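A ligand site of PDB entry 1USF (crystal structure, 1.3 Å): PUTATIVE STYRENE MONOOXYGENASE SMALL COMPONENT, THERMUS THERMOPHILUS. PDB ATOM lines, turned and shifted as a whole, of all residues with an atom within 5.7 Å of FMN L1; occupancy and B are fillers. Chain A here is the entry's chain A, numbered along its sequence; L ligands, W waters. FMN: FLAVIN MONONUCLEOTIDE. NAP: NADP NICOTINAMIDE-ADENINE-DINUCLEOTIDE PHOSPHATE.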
ATOM      1  N   PRO A  21      39.777  28.926  -8.180  1.00  0.00           N
ATOM      2  CA  PRO A  21      38.403  29.125  -7.716  1.00  0.00           C
ATOM      3  C   PRO A  21      38.333  30.349  -6.817  1.00  0.00           C
ATOM      4  O   PRO A  21      39.183  30.529  -5.932  1.00  0.00           O
ATOM      5  CB  PRO A  21      38.111  27.839  -6.957  1.00  0.00           C
ATOM      6  CG  PRO A  21      39.437  27.517  -6.341  1.00  0.00           C
ATOM      7  CD  PRO A  21      40.420  27.811  -7.471  1.00  0.00           C
ATOM      8  N   ASN A  33      27.840  33.242   4.415  1.00  0.00           N
ATOM      9  CA  ASN A  33      27.974  32.042   3.612  1.00  0.00           C
ATOM     10  C   ASN A  33      29.191  32.186   2.687  1.00  0.00           C
ATOM     11  O   ASN A  33      29.580  33.292   2.344  1.00  0.00           O
ATOM     12  CB  ASN A  33      26.710  31.794   2.759  1.00  0.00           C
ATOM     13  CG  ASN A  33      26.588  30.347   2.290  1.00  0.00           C
ATOM     14  OD1 ASN A  33      26.605  29.431   3.104  1.00  0.00           O
ATOM     15  ND2 ASN A  33      26.478  30.149   0.988  1.00  0.00           N
ATOM     16  N   PHE A  34      29.800  31.048   2.331  1.00  0.00           N
ATOM     17  CA  PHE A  34      30.943  31.024   1.422  1.00  0.00           C
ATOM     18  C   PHE A  34      30.725  29.954   0.381  1.00  0.00           C
ATOM     19  O   PHE A  34      30.206  28.879   0.686  1.00  0.00           O
ATOM     20  CB  PHE A  34      32.249  30.723   2.146  1.00  0.00           C
ATOM     21  CG  PHE A  34      32.611  31.738   3.168  1.00  0.00           C
ATOM     22  CD1 PHE A  34      32.398  31.482   4.514  1.00  0.00           C
ATOM     23  CD2 PHE A  34      33.191  32.937   2.793  1.00  0.00           C
ATOM     24  CE1 PHE A  34      32.754  32.404   5.464  1.00  0.00           C
ATOM     25  CE2 PHE A  34      33.554  33.871   3.746  1.00  0.00           C
ATOM     26  CZ  PHE A  34      33.334  33.603   5.088  1.00  0.00           C
ATOM     27  N   CYS A  35      31.127  30.284  -0.832  1.00  0.00           N
ATOM     28  CA  CYS A  35      30.937  29.458  -2.012  1.00  0.00           C
ATOM     29  C   CYS A  35      32.039  29.545  -3.101  1.00  0.00           C
ATOM     30  O   CYS A  35      32.210  30.576  -3.726  1.00  0.00           O
ATOM     31  CB  CYS A  35      29.575  29.850  -2.597  1.00  0.00           C
ATOM     32  SG  CYS A  35      29.107  29.207  -4.209  1.00  0.00           S
ATOM     33  N   PRO A  36      32.809  28.468  -3.313  1.00  0.00           N
ATOM     34  CA  PRO A  36      33.831  28.587  -4.354  1.00  0.00           C
ATOM     35  C   PRO A  36      33.175  28.699  -5.721  1.00  0.00           C
ATOM     36  O   PRO A  36      32.113  28.116  -5.959  1.00  0.00           O
ATOM     37  CB  PRO A  36      34.643  27.309  -4.189  1.00  0.00           C
ATOM     38  CG  PRO A  36      33.643  26.330  -3.711  1.00  0.00           C
ATOM     39  CD  PRO A  36      32.880  27.139  -2.678  1.00  0.00           C
ATOM     40  N   ALA A  37      33.811  29.449  -6.606  1.00  0.00           N
ATOM     41  CA  ALA A  37      33.304  29.635  -7.954  1.00  0.00           C
ATOM     42  C   ALA A  37      34.481  29.612  -8.926  1.00  0.00           C
ATOM     43  O   ALA A  37      35.270  30.558  -8.971  1.00  0.00           O
ATOM     44  CB  ALA A  37      32.563  30.970  -8.056  1.00  0.00           C
ATOM     45  N   VAL A  38      34.600  28.530  -9.693  1.00  0.00           N
ATOM     46  CA  VAL A  38      35.690  28.427 -10.653  1.00  0.00           C
ATOM     47  C   VAL A  38      35.333  29.217 -11.916  1.00  0.00           C
ATOM     48  O   VAL A  38      36.199  29.565 -12.713  1.00  0.00           O
ATOM     49  CB  VAL A  38      36.013  26.928 -11.002  1.00  0.00           C
ATOM     50  CG1 VAL A  38      34.851  26.294 -11.762  1.00  0.00           C
ATOM     51  CG2 VAL A  38      37.313  26.850 -11.803  1.00  0.00           C
ATOM     52  N   TRP A  39      34.042  29.499 -12.088  1.00  0.00           N
ATOM     53  CA  TRP A  39      33.625  30.299 -13.221  1.00  0.00           C
ATOM     54  C   TRP A  39      33.699  31.758 -12.776  1.00  0.00           C
ATOM     55  O   TRP A  39      32.707  32.359 -12.331  1.00  0.00           O
ATOM     56  CB  TRP A  39      32.203  29.941 -13.658  1.00  0.00           C
ATOM     57  CG  TRP A  39      32.119  28.646 -14.425  1.00  0.00           C
ATOM     58  CD1 TRP A  39      33.138  27.784 -14.703  1.00  0.00           C
ATOM     59  CD2 TRP A  39      30.940  28.073 -14.996  1.00  0.00           C
ATOM     60  NE1 TRP A  39      32.664  26.698 -15.410  1.00  0.00           N
ATOM     61  CE2 TRP A  39      31.314  26.851 -15.602  1.00  0.00           C
ATOM     62  CE3 TRP A  39      29.589  28.464 -15.051  1.00  0.00           C
ATOM     63  CZ2 TRP A  39      30.396  26.023 -16.249  1.00  0.00           C
ATOM     64  CZ3 TRP A  39      28.679  27.631 -15.696  1.00  0.00           C
ATOM     65  CH2 TRP A  39      29.089  26.428 -16.294  1.00  0.00           C
ATOM     66  N   ASN A  40      34.901  32.308 -12.853  1.00  0.00           N
ATOM     67  CA  ASN A  40      35.140  33.699 -12.481  1.00  0.00           C
ATOM     68  C   ASN A  40      36.125  34.262 -13.492  1.00  0.00           C
ATOM     69  O   ASN A  40      36.891  33.513 -14.115  1.00  0.00           O
ATOM     70  CB  ASN A  40      35.706  33.811 -11.050  1.00  0.00           C
ATOM     71  CG  ASN A  40      37.114  33.265 -10.919  1.00  0.00           C
ATOM     72  OD1 ASN A  40      38.088  33.950 -11.216  1.00  0.00           O
ATOM     73  ND2 ASN A  40      37.231  32.033 -10.454  1.00  0.00           N
ATOM     74  N   SER A  53      30.135  33.525 -11.913  1.00  0.00           N
ATOM     75  CA  SER A  53      28.924  32.930 -12.467  1.00  0.00           C
ATOM     76  C   SER A  53      28.371  31.915 -11.478  1.00  0.00           C
ATOM     77  O   SER A  53      28.977  30.872 -11.255  1.00  0.00           O
ATOM     78  CB  SER A  53      29.267  32.252 -13.801  1.00  0.00           C
ATOM     79  OG  SER A  53      28.115  31.675 -14.385  1.00  0.00           O
ATOM     80  N   ILE A  54      27.199  32.227 -10.917  1.00  0.00           N
ATOM     81  CA  ILE A  54      26.567  31.397  -9.902  1.00  0.00           C
ATOM     82  C   ILE A  54      25.211  30.837 -10.319  1.00  0.00           C
ATOM     83  O   ILE A  54      24.353  31.571 -10.806  1.00  0.00           O
ATOM     84  CB  ILE A  54      26.361  32.218  -8.601  1.00  0.00           C
ATOM     85  CG1 ILE A  54      27.684  32.874  -8.180  1.00  0.00           C
ATOM     86  CG2 ILE A  54      25.797  31.326  -7.497  1.00  0.00           C
ATOM     87  CD1 ILE A  54      28.805  31.907  -7.889  1.00  0.00           C
ATOM     88  N   SER A  55      25.008  29.551 -10.089  1.00  0.00           N
ATOM     89  CA  SER A  55      23.747  28.909 -10.432  1.00  0.00           C
ATOM     90  C   SER A  55      22.643  29.348  -9.474  1.00  0.00           C
ATOM     91  O   SER A  55      22.860  29.525  -8.278  1.00  0.00           O
ATOM     92  CB  SER A  55      23.889  27.389 -10.335  1.00  0.00           C
ATOM     93  OG  SER A  55      22.607  26.762 -10.296  1.00  0.00           O
ATOM     94  N   LYS A  57      20.635  27.707  -8.262  1.00  0.00           N
ATOM     95  CA  LYS A  57      20.421  26.581  -7.351  1.00  0.00           C
ATOM     96  C   LYS A  57      21.229  26.720  -6.060  1.00  0.00           C
ATOM     97  O   LYS A  57      20.971  26.027  -5.078  1.00  0.00           O
ATOM     98  CB  LYS A  57      20.806  25.260  -8.016  1.00  0.00           C
ATOM     99  CG  LYS A  57      19.872  24.805  -9.135  1.00  0.00           C
ATOM    100  CD  LYS A  57      20.285  23.433  -9.642  1.00  0.00           C
ATOM    101  CE  LYS A  57      19.270  22.828 -10.602  1.00  0.00           C
ATOM    102  NZ  LYS A  57      19.302  23.447 -11.959  1.00  0.00           N
ATOM    103  N   ARG A  58      22.215  27.608  -6.058  1.00  0.00           N
ATOM    104  CA  ARG A  58      23.040  27.797  -4.870  1.00  0.00           C
ATOM    105  C   ARG A  58      22.356  28.718  -3.880  1.00  0.00           C
ATOM    106  O   ARG A  58      21.682  29.672  -4.251  1.00  0.00           O
ATOM    107  CB  ARG A  58      24.402  28.413  -5.229  1.00  0.00           C
ATOM    108  CG  ARG A  58      25.073  27.855  -6.487  1.00  0.00           C
ATOM    109  CD  ARG A  58      25.299  26.360  -6.439  1.00  0.00           C
ATOM    110  NE  ARG A  58      26.106  25.951  -7.591  1.00  0.00           N
ATOM    111  CZ  ARG A  58      25.858  24.891  -8.352  1.00  0.00           C
ATOM    112  NH1 ARG A  58      24.812  24.102  -8.102  1.00  0.00           N
ATOM    113  NH2 ARG A  58      26.637  24.634  -9.394  1.00  0.00           N
ATOM    114  N   PHE A  59      22.550  28.435  -2.600  1.00  0.00           N
ATOM    115  CA  PHE A  59      21.992  29.246  -1.534  1.00  0.00           C
ATOM    116  C   PHE A  59      22.602  30.643  -1.680  1.00  0.00           C
ATOM    117  O   PHE A  59      21.946  31.660  -1.445  1.00  0.00           O
ATOM    118  CB  PHE A  59      22.367  28.624  -0.187  1.00  0.00           C
ATOM    119  CG  PHE A  59      21.861  29.369   1.007  1.00  0.00           C
ATOM    120  CD1 PHE A  59      22.752  29.865   1.954  1.00  0.00           C
ATOM    121  CD2 PHE A  59      20.498  29.555   1.208  1.00  0.00           C
ATOM    122  CE1 PHE A  59      22.287  30.518   3.094  1.00  0.00           C
ATOM    123  CE2 PHE A  59      20.025  30.213   2.346  1.00  0.00           C
ATOM    124  CZ  PHE A  59      20.923  30.698   3.286  1.00  0.00           C
ATOM    125  N   THR A  60      23.857  30.681  -2.121  1.00  0.00           N
ATOM    126  CA  THR A  60      24.593  31.919  -2.303  1.00  0.00           C
ATOM    127  C   THR A  60      23.938  32.871  -3.300  1.00  0.00           C
ATOM    128  O   THR A  60      24.038  34.093  -3.150  1.00  0.00           O
ATOM    129  CB  THR A  60      26.045  31.614  -2.771  1.00  0.00           C
ATOM    130  OG1 THR A  60      26.719  30.853  -1.764  1.00  0.00           O
ATOM    131  CG2 THR A  60      26.832  32.895  -3.021  1.00  0.00           C
ATOM    132  N   HIS A  61      23.276  32.328  -4.315  1.00  0.00           N
ATOM    133  CA  HIS A  61      22.618  33.142  -5.333  1.00  0.00           C
ATOM    134  C   HIS A  61      21.629  34.130  -4.712  1.00  0.00           C
ATOM    135  O   HIS A  61      21.712  35.330  -4.958  1.00  0.00           O
ATOM    136  CB  HIS A  61      21.914  32.220  -6.348  1.00  0.00           C
ATOM    137  CG  HIS A  61      21.343  32.942  -7.532  1.00  0.00           C
ATOM    138  ND1 HIS A  61      20.142  33.606  -7.488  1.00  0.00           N
ATOM    139  CD2 HIS A  61      21.800  33.058  -8.798  1.00  0.00           C
ATOM    140  CE1 HIS A  61      19.884  34.122  -8.678  1.00  0.00           C
ATOM    141  NE2 HIS A  61      20.874  33.799  -9.493  1.00  0.00           N
ATOM    142  N   VAL A  83      38.372  24.712   1.070  1.00  0.00           N
ATOM    143  CA  VAL A  83      37.666  25.189  -0.114  1.00  0.00           C
ATOM    144  C   VAL A  83      36.752  24.092  -0.656  1.00  0.00           C
ATOM    145  O   VAL A  83      35.589  24.341  -0.988  1.00  0.00           O
ATOM    146  CB  VAL A  83      38.673  25.637  -1.211  1.00  0.00           C
ATOM    147  CG1 VAL A  83      37.922  25.987  -2.501  1.00  0.00           C
ATOM    148  CG2 VAL A  83      39.465  26.842  -0.721  1.00  0.00           C
ATOM    149  N   HIS A  84      37.269  22.874  -0.705  1.00  0.00           N
ATOM    150  CA  HIS A  84      36.480  21.745  -1.195  1.00  0.00           C
ATOM    151  C   HIS A  84      35.262  21.512  -0.309  1.00  0.00           C
ATOM    152  O   HIS A  84      34.170  21.215  -0.811  1.00  0.00           O
ATOM    153  CB  HIS A  84      37.317  20.478  -1.240  1.00  0.00           C
ATOM    154  CG  HIS A  84      36.539  19.276  -1.687  1.00  0.00           C
ATOM    155  ND1 HIS A  84      36.027  19.149  -2.962  1.00  0.00           N
ATOM    156  CD2 HIS A  84      36.158  18.166  -1.014  1.00  0.00           C
ATOM    157  CE1 HIS A  84      35.372  18.011  -3.051  1.00  0.00           C
ATOM    158  NE2 HIS A  84      35.425  17.394  -1.881  1.00  0.00           N
ATOM    159  N   LEU A  86      33.650  23.728   1.485  1.00  0.00           N
ATOM    160  CA  LEU A  86      32.714  24.810   1.231  1.00  0.00           C
ATOM    161  C   LEU A  86      31.963  24.612  -0.089  1.00  0.00           C
ATOM    162  O   LEU A  86      30.835  25.075  -0.250  1.00  0.00           O
ATOM    163  CB  LEU A  86      33.449  26.157   1.219  1.00  0.00           C
ATOM    164  CG  LEU A  86      34.047  26.578   2.563  1.00  0.00           C
ATOM    165  CD1 LEU A  86      34.970  27.769   2.364  1.00  0.00           C
ATOM    166  CD2 LEU A  86      32.929  26.934   3.537  1.00  0.00           C
ATOM    167  N   GLY A  87      32.597  23.928  -1.030  1.00  0.00           N
ATOM    168  CA  GLY A  87      31.968  23.687  -2.315  1.00  0.00           C
ATOM    169  C   GLY A  87      31.262  22.337  -2.399  1.00  0.00           C
ATOM    170  O   GLY A  87      30.798  21.959  -3.467  1.00  0.00           O
ATOM    171  N   SER A  88      31.199  21.620  -1.284  1.00  0.00           N
ATOM    172  CA  SER A  88      30.559  20.311  -1.247  1.00  0.00           C
ATOM    173  C   SER A  88      29.379  20.259  -0.276  1.00  0.00           C
ATOM    174  O   SER A  88      28.780  19.205  -0.069  1.00  0.00           O
ATOM    175  CB  SER A  88      31.584  19.224  -0.882  1.00  0.00           C
ATOM    176  OG  SER A  88      32.267  19.539   0.316  1.00  0.00           O
ATOM    177  N   HIS A  89      29.059  21.408   0.322  1.00  0.00           N
ATOM    178  CA  HIS A  89      27.941  21.513   1.249  1.00  0.00           C
ATOM    179  C   HIS A  89      27.231  22.836   1.021  1.00  0.00           C
ATOM    180  O   HIS A  89      27.849  23.806   0.569  1.00  0.00           O
ATOM    181  CB  HIS A  89      28.415  21.415   2.700  1.00  0.00           C
ATOM    182  CG  HIS A  89      29.089  20.122   3.031  1.00  0.00           C
ATOM    183  ND1 HIS A  89      30.404  19.874   2.721  1.00  0.00           N
ATOM    184  CD2 HIS A  89      28.615  18.999   3.606  1.00  0.00           C
ATOM    185  CE1 HIS A  89      30.716  18.647   3.102  1.00  0.00           C
ATOM    186  NE2 HIS A  89      29.642  18.089   3.638  1.00  0.00           N
ATOM    187  N   SER A  90      25.943  22.889   1.329  1.00  0.00           N
ATOM    188  CA  SER A  90      25.152  24.096   1.135  1.00  0.00           C
ATOM    189  C   SER A  90      24.758  24.792   2.428  1.00  0.00           C
ATOM    190  O   SER A  90      24.532  24.144   3.450  1.00  0.00           O
ATOM    191  CB  SER A  90      23.875  23.772   0.353  1.00  0.00           C
ATOM    192  OG  SER A  90      23.009  24.895   0.289  1.00  0.00           O
ATOM    193  N   GLY A  91      24.651  26.116   2.341  1.00  0.00           N
ATOM    194  CA  GLY A  91      24.257  26.905   3.484  1.00  0.00           C
ATOM    195  C   GLY A  91      22.819  26.616   3.853  1.00  0.00           C
ATOM    196  O   GLY A  91      22.319  27.079   4.878  1.00  0.00           O
ATOM    197  N   ARG A  92      22.133  25.849   3.012  1.00  0.00           N
ATOM    198  CA  ARG A  92      20.745  25.470   3.301  1.00  0.00           C
ATOM    199  C   ARG A  92      20.744  24.431   4.417  1.00  0.00           C
ATOM    200  O   ARG A  92      19.750  24.270   5.114  1.00  0.00           O
ATOM    201  CB  ARG A  92      20.070  24.850   2.076  1.00  0.00           C
ATOM    202  CG  ARG A  92      19.628  25.814   0.988  1.00  0.00           C
ATOM    203  CD  ARG A  92      18.869  25.051  -0.094  1.00  0.00           C
ATOM    204  NE  ARG A  92      19.706  24.040  -0.730  1.00  0.00           N
ATOM    205  CZ  ARG A  92      20.596  24.297  -1.686  1.00  0.00           C
ATOM    206  NH1 ARG A  92      20.746  25.540  -2.131  1.00  0.00           N
ATOM    207  NH2 ARG A  92      21.337  23.317  -2.189  1.00  0.00           N
ATOM    208  N   LYS A  96      28.003  27.648   7.143  1.00  0.00           N
ATOM    209  CA  LYS A  96      29.389  27.801   6.710  1.00  0.00           C
ATOM    210  C   LYS A  96      29.984  29.091   7.255  1.00  0.00           C
ATOM    211  O   LYS A  96      31.194  29.320   7.149  1.00  0.00           O
ATOM    212  CB  LYS A  96      29.464  27.740   5.173  1.00  0.00           C
ATOM    213  CG  LYS A  96      29.203  26.340   4.609  1.00  0.00           C
ATOM    214  CD  LYS A  96      29.485  26.230   3.101  1.00  0.00           C
ATOM    215  CE  LYS A  96      28.297  26.645   2.259  1.00  0.00           C
ATOM    216  NZ  LYS A  96      28.600  26.544   0.791  1.00  0.00           N
ATOM    217  N   HIS A 131      23.269  29.643 -15.458  1.00  0.00           N
ATOM    218  CA  HIS A 131      23.997  30.366 -14.408  1.00  0.00           C
ATOM    219  C   HIS A 131      23.819  31.863 -14.604  1.00  0.00           C
ATOM    220  O   HIS A 131      23.597  32.340 -15.716  1.00  0.00           O
ATOM    221  CB  HIS A 131      25.508  30.070 -14.441  1.00  0.00           C
ATOM    222  CG  HIS A 131      25.913  28.786 -13.802  1.00  0.00           C
ATOM    223  ND1 HIS A 131      25.494  27.550 -14.258  1.00  0.00           N
ATOM    224  CD2 HIS A 131      26.780  28.528 -12.793  1.00  0.00           C
ATOM    225  CE1 HIS A 131      26.082  26.601 -13.562  1.00  0.00           C
ATOM    226  NE2 HIS A 131      26.868  27.159 -12.665  1.00  0.00           N
ATOM    227  N   TYR A 162      41.564  24.307  -9.685  1.00  0.00           N
ATOM    228  CA  TYR A 162      40.466  23.345  -9.700  1.00  0.00           C
ATOM    229  C   TYR A 162      40.320  22.770 -11.098  1.00  0.00           C
ATOM    230  O   TYR A 162      40.246  23.516 -12.073  1.00  0.00           O
ATOM    231  CB  TYR A 162      39.156  24.020  -9.286  1.00  0.00           C
ATOM    232  CG  TYR A 162      38.000  23.056  -9.162  1.00  0.00           C
ATOM    233  CD1 TYR A 162      38.114  21.914  -8.363  1.00  0.00           C
ATOM    234  CD2 TYR A 162      36.783  23.287  -9.806  1.00  0.00           C
ATOM    235  CE1 TYR A 162      37.037  21.044  -8.200  1.00  0.00           C
ATOM    236  CE2 TYR A 162      35.699  22.422  -9.646  1.00  0.00           C
ATOM    237  CZ  TYR A 162      35.840  21.304  -8.841  1.00  0.00           C
ATOM    238  OH  TYR A 162      34.776  20.448  -8.641  1.00  0.00           O
ATOM    239  N   TYR A 168      41.794  18.766  -7.528  1.00  0.00           N
ATOM    240  CA  TYR A 168      42.555  19.996  -7.366  1.00  0.00           C
ATOM    241  C   TYR A 168      44.046  19.804  -7.625  1.00  0.00           C
ATOM    242  O   TYR A 168      44.557  18.687  -7.629  1.00  0.00           O
ATOM    243  CB  TYR A 168      42.409  20.556  -5.960  1.00  0.00           C
ATOM    244  CG  TYR A 168      40.990  20.814  -5.538  1.00  0.00           C
ATOM    245  CD1 TYR A 168      40.145  19.761  -5.197  1.00  0.00           C
ATOM    246  CD2 TYR A 168      40.481  22.114  -5.493  1.00  0.00           C
ATOM    247  CE1 TYR A 168      38.834  19.988  -4.827  1.00  0.00           C
ATOM    248  CE2 TYR A 168      39.154  22.352  -5.128  1.00  0.00           C
ATOM    249  CZ  TYR A 168      38.339  21.283  -4.793  1.00  0.00           C
ATOM    250  OH  TYR A 168      37.033  21.494  -4.438  1.00  0.00           O
HETATM  251  N1  FMN L   1      28.940  26.667  -8.409  1.00  0.00           N
HETATM  252  C2  FMN L   1      28.534  27.667  -9.205  1.00  0.00           C
HETATM  253  O2  FMN L   1      27.378  28.084  -9.381  1.00  0.00           O
HETATM  254  N3  FMN L   1      29.552  28.393  -9.991  1.00  0.00           N
HETATM  255  C4  FMN L   1      30.944  28.066  -9.920  1.00  0.00           C
HETATM  256  O4  FMN L   1      31.679  28.761 -10.642  1.00  0.00           O
HETATM  257  C4A FMN L   1      31.294  27.025  -9.081  1.00  0.00           C
HETATM  258  N5  FMN L   1      32.551  26.708  -9.001  1.00  0.00           N
HETATM  259  C5A FMN L   1      32.978  25.749  -8.056  1.00  0.00           C
HETATM  260  C6  FMN L   1      34.343  25.476  -7.815  1.00  0.00           C
HETATM  261  C7  FMN L   1      34.729  24.483  -6.821  1.00  0.00           C
HETATM  262  C7M FMN L   1      36.202  24.204  -6.578  1.00  0.00           C
HETATM  263  C8  FMN L   1      33.697  23.754  -6.079  1.00  0.00           C
HETATM  264  C8M FMN L   1      34.098  22.744  -5.087  1.00  0.00           C
HETATM  265  C9  FMN L   1      32.363  24.021  -6.308  1.00  0.00           C
HETATM  266  C9A FMN L   1      31.919  25.041  -7.300  1.00  0.00           C
HETATM  267  N10 FMN L   1      30.557  25.254  -7.445  1.00  0.00           N
HETATM  268  C10 FMN L   1      30.223  26.284  -8.280  1.00  0.00           C
HETATM  269  C1' FMN L   1      29.471  24.719  -6.614  1.00  0.00           C
HETATM  270  C2' FMN L   1      29.199  25.449  -5.309  1.00  0.00           C
HETATM  271  O2' FMN L   1      30.404  25.932  -4.745  1.00  0.00           O
HETATM  272  C3' FMN L   1      28.550  24.426  -4.433  1.00  0.00           C
HETATM  273  O3' FMN L   1      27.248  24.048  -4.979  1.00  0.00           O
HETATM  274  C4' FMN L   1      28.265  24.961  -3.007  1.00  0.00           C
HETATM  275  O4' FMN L   1      28.035  23.884  -2.136  1.00  0.00           O
HETATM  276  C5' FMN L   1      27.071  25.948  -3.020  1.00  0.00           C
HETATM  277  O5' FMN L   1      26.960  26.393  -1.666  1.00  0.00           O
HETATM  278  P   FMN L   1      25.671  27.185  -1.255  1.00  0.00           P
HETATM  279  O1P FMN L   1      24.420  26.323  -1.524  1.00  0.00           O
HETATM  280  O2P FMN L   1      25.612  28.450  -2.029  1.00  0.00           O
HETATM  281  O3P FMN L   1      25.790  27.496   0.236  1.00  0.00           O
HETATM  282  PA  NAP L   2      26.300  19.122 -10.799  1.00  0.00           P
HETATM  283  O1A NAP L   2      25.203  20.141 -11.290  1.00  0.00           O
HETATM  284  O2A NAP L   2      26.917  18.433 -11.900  1.00  0.00           O
HETATM  285  O5B NAP L   2      27.417  20.168 -10.214  1.00  0.00           O
HETATM  286  C5B NAP L   2      27.243  20.717  -8.904  1.00  0.00           C
HETATM  287  C4B NAP L   2      28.396  21.713  -8.705  1.00  0.00           C
HETATM  288  O4B NAP L   2      29.324  21.034  -7.836  1.00  0.00           O
HETATM  289  C3B NAP L   2      29.179  22.131  -9.923  1.00  0.00           C
HETATM  290  O3B NAP L   2      29.548  23.532  -9.819  1.00  0.00           O
HETATM  291  C2B NAP L   2      30.399  21.299  -9.961  1.00  0.00           C
HETATM  292  O2B NAP L   2      31.565  21.860 -10.545  1.00  0.00           O
HETATM  293  C1B NAP L   2      30.552  20.903  -8.526  1.00  0.00           C
HETATM  294  N9A NAP L   2      31.054  19.506  -8.370  1.00  0.00           N
HETATM  295  C8A NAP L   2      30.810  18.376  -9.183  1.00  0.00           C
HETATM  296  N7A NAP L   2      31.397  17.303  -8.681  1.00  0.00           N
HETATM  297  C5A NAP L   2      32.048  17.721  -7.553  1.00  0.00           C
HETATM  298  C6A NAP L   2      32.819  17.066  -6.575  1.00  0.00           C
HETATM  299  N6A NAP L   2      33.056  15.757  -6.664  1.00  0.00           N
HETATM  300  N1A NAP L   2      33.336  17.786  -5.544  1.00  0.00           N
HETATM  301  C2A NAP L   2      33.110  19.121  -5.471  1.00  0.00           C
HETATM  302  N3A NAP L   2      32.394  19.828  -6.347  1.00  0.00           N
HETATM  303  C4A NAP L   2      31.866  19.060  -7.370  1.00  0.00           C
HETATM  304  O3  NAP L   2      25.640  18.380  -9.657  1.00  0.00           O
HETATM  305  P2B NAP L   2      32.426  21.241 -11.659  1.00  0.00           P
HETATM  306  O1X NAP L   2      33.231  20.239 -10.968  1.00  0.00           O
HETATM  307  O2X NAP L   2      33.223  22.352 -12.241  1.00  0.00           O
HETATM  308  O3X NAP L   2      31.527  20.592 -12.723  1.00  0.00           O
HETATM  309  O   HOH W   1      25.840  22.401  -2.539  1.00  0.00           O
HETATM  310  O   HOH W   2      23.977  24.326  -3.220  1.00  0.00           O
HETATM  311  O   HOH W   3      26.798  21.162  -4.840  1.00  0.00           O
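Residues that only touch FMN L1: Ala 37 (3.2 Å), Tyr 168 (3.3 Å), Tyr 162 (3.4 Å), Ile 54 (3.5 Å), Gly 87 (3.5 Å), Leu 86 (3.6 Å) and Ser 88 (3.98 Å).
Of the 30 residues printed, 23 come within 4 Å of FMN L1.
The nearest printed residue that does not touch FMN L1 is Pro 21 (4.1 Å).
Water W2 bridges O1P of FMN L1 (2.7 Å) and NH2 of Arg 92 (3.0 Å).
N1 of FMN L1 lies close to O3B of NAP L2 (3.5 Å).
The backbone carbonyl oxygen (O) of Pro 36 sits at hydrogen-bond distance from an oxygen (O2') of FMN L1 (3.0 Å).
The backbone NH (N) of Trp 39 lies within hydrogen-bond range of an oxygen (O4) of FMN L1, 2.9 Å away.
A nitrogen (N1) of FMN L1 sits at hydrogen-bond distance from the guanidinium group (NE) of Arg 58 (3.0 Å).
An oxygen (O2) of FMN L1 is in hydrogen-bond range of the backbone NH (N) of Ser 55.
The side-chain hydroxyl of Ser 90 is in hydrogen-bond range of an oxygen (O1P) of FMN L1 (2.7 Å).
The guanidinium group (NH1) of Arg 92 is in salt-bridge range of an oxygen (O1P) of FMN L1, at 3.8 Å.
The backbone carbonyl oxygen of Ser 53 is in hydrogen-bond range of a nitrogen (N3) of FMN L1, at 2.8 Å.
The backbone NH (N) of Gly 91 is in hydrogen-bond range of an oxygen (O3P) of FMN L1.
N of Phe 59 is in hydrogen-bond range of O1P of FMN L1 (3.0 Å).
The side-chain amino group of Lys 96 is in salt-bridge range of an oxygen (O3P) of FMN L1.
The backbone NH (N) of Thr 60 lies within hydrogen-bond range of an oxygen (O2P) of FMN L1.
NH2 of Arg 58 is in hydrogen-bond range of O3B of NAP L2 (3.1 Å).
An oxygen (O3P) of FMN L1 is in hydrogen-bond range of the side-chain amide nitrogen of Asn 33 (2.8 Å).
A ring nitrogen (NE2) of His 131 lies within hydrogen-bond range of an oxygen (O2) of FMN L1 (3.4 Å).
N5 of FMN L1 is in hydrogen-bond range of N of Val 38 (2.8 Å).
The side-chain hydroxyl of Tyr 162 sits at hydrogen-bond distance from an oxygen (O1X) of NAP L2, 2.8 Å away.
The side-chain sulfur of Cys 35 sits at hydrogen-bond distance from an oxygen (O2') of FMN L1 (3.6 Å).
The side-chain hydroxyl (OG1) of Thr 60 is in hydrogen-bond range of an oxygen (O2P) of FMN L1, at 2.7 Å.
O of His 89 is in hydrogen-bond range of O4' of FMN L1.
OG1 of Thr 60 sits close to SG of Cys 35 (3.8 Å).
The backbone NH (N) of Ser 53 lies within hydrogen-bond range of the backbone carbonyl oxygen (O) of Trp 39.
O of Leu 86 is in hydrogen-bond range of NZ of Lys 96 (2.9 Å).
The guanidinium group (NH1) of Arg 92 is in hydrogen-bond range of the backbone carbonyl oxygen (O) of Lys 57 (3.0 Å).
The backbone carbonyl oxygen (O) of His 84 sits at hydrogen-bond distance from the side-chain hydroxyl (OG) of Ser 88 (2.8 Å).
The side-chain hydroxyl (OG) of Ser 88 lies within hydrogen-bond range of a ring nitrogen (ND1) of His 89, 3.1 Å away.
O of Ala 37 lies within hydrogen-bond range of ND2 of Asn 40, 2.9 Å away.
OG of Ser 55 lies close to N of Lys 57 (3.0 Å).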
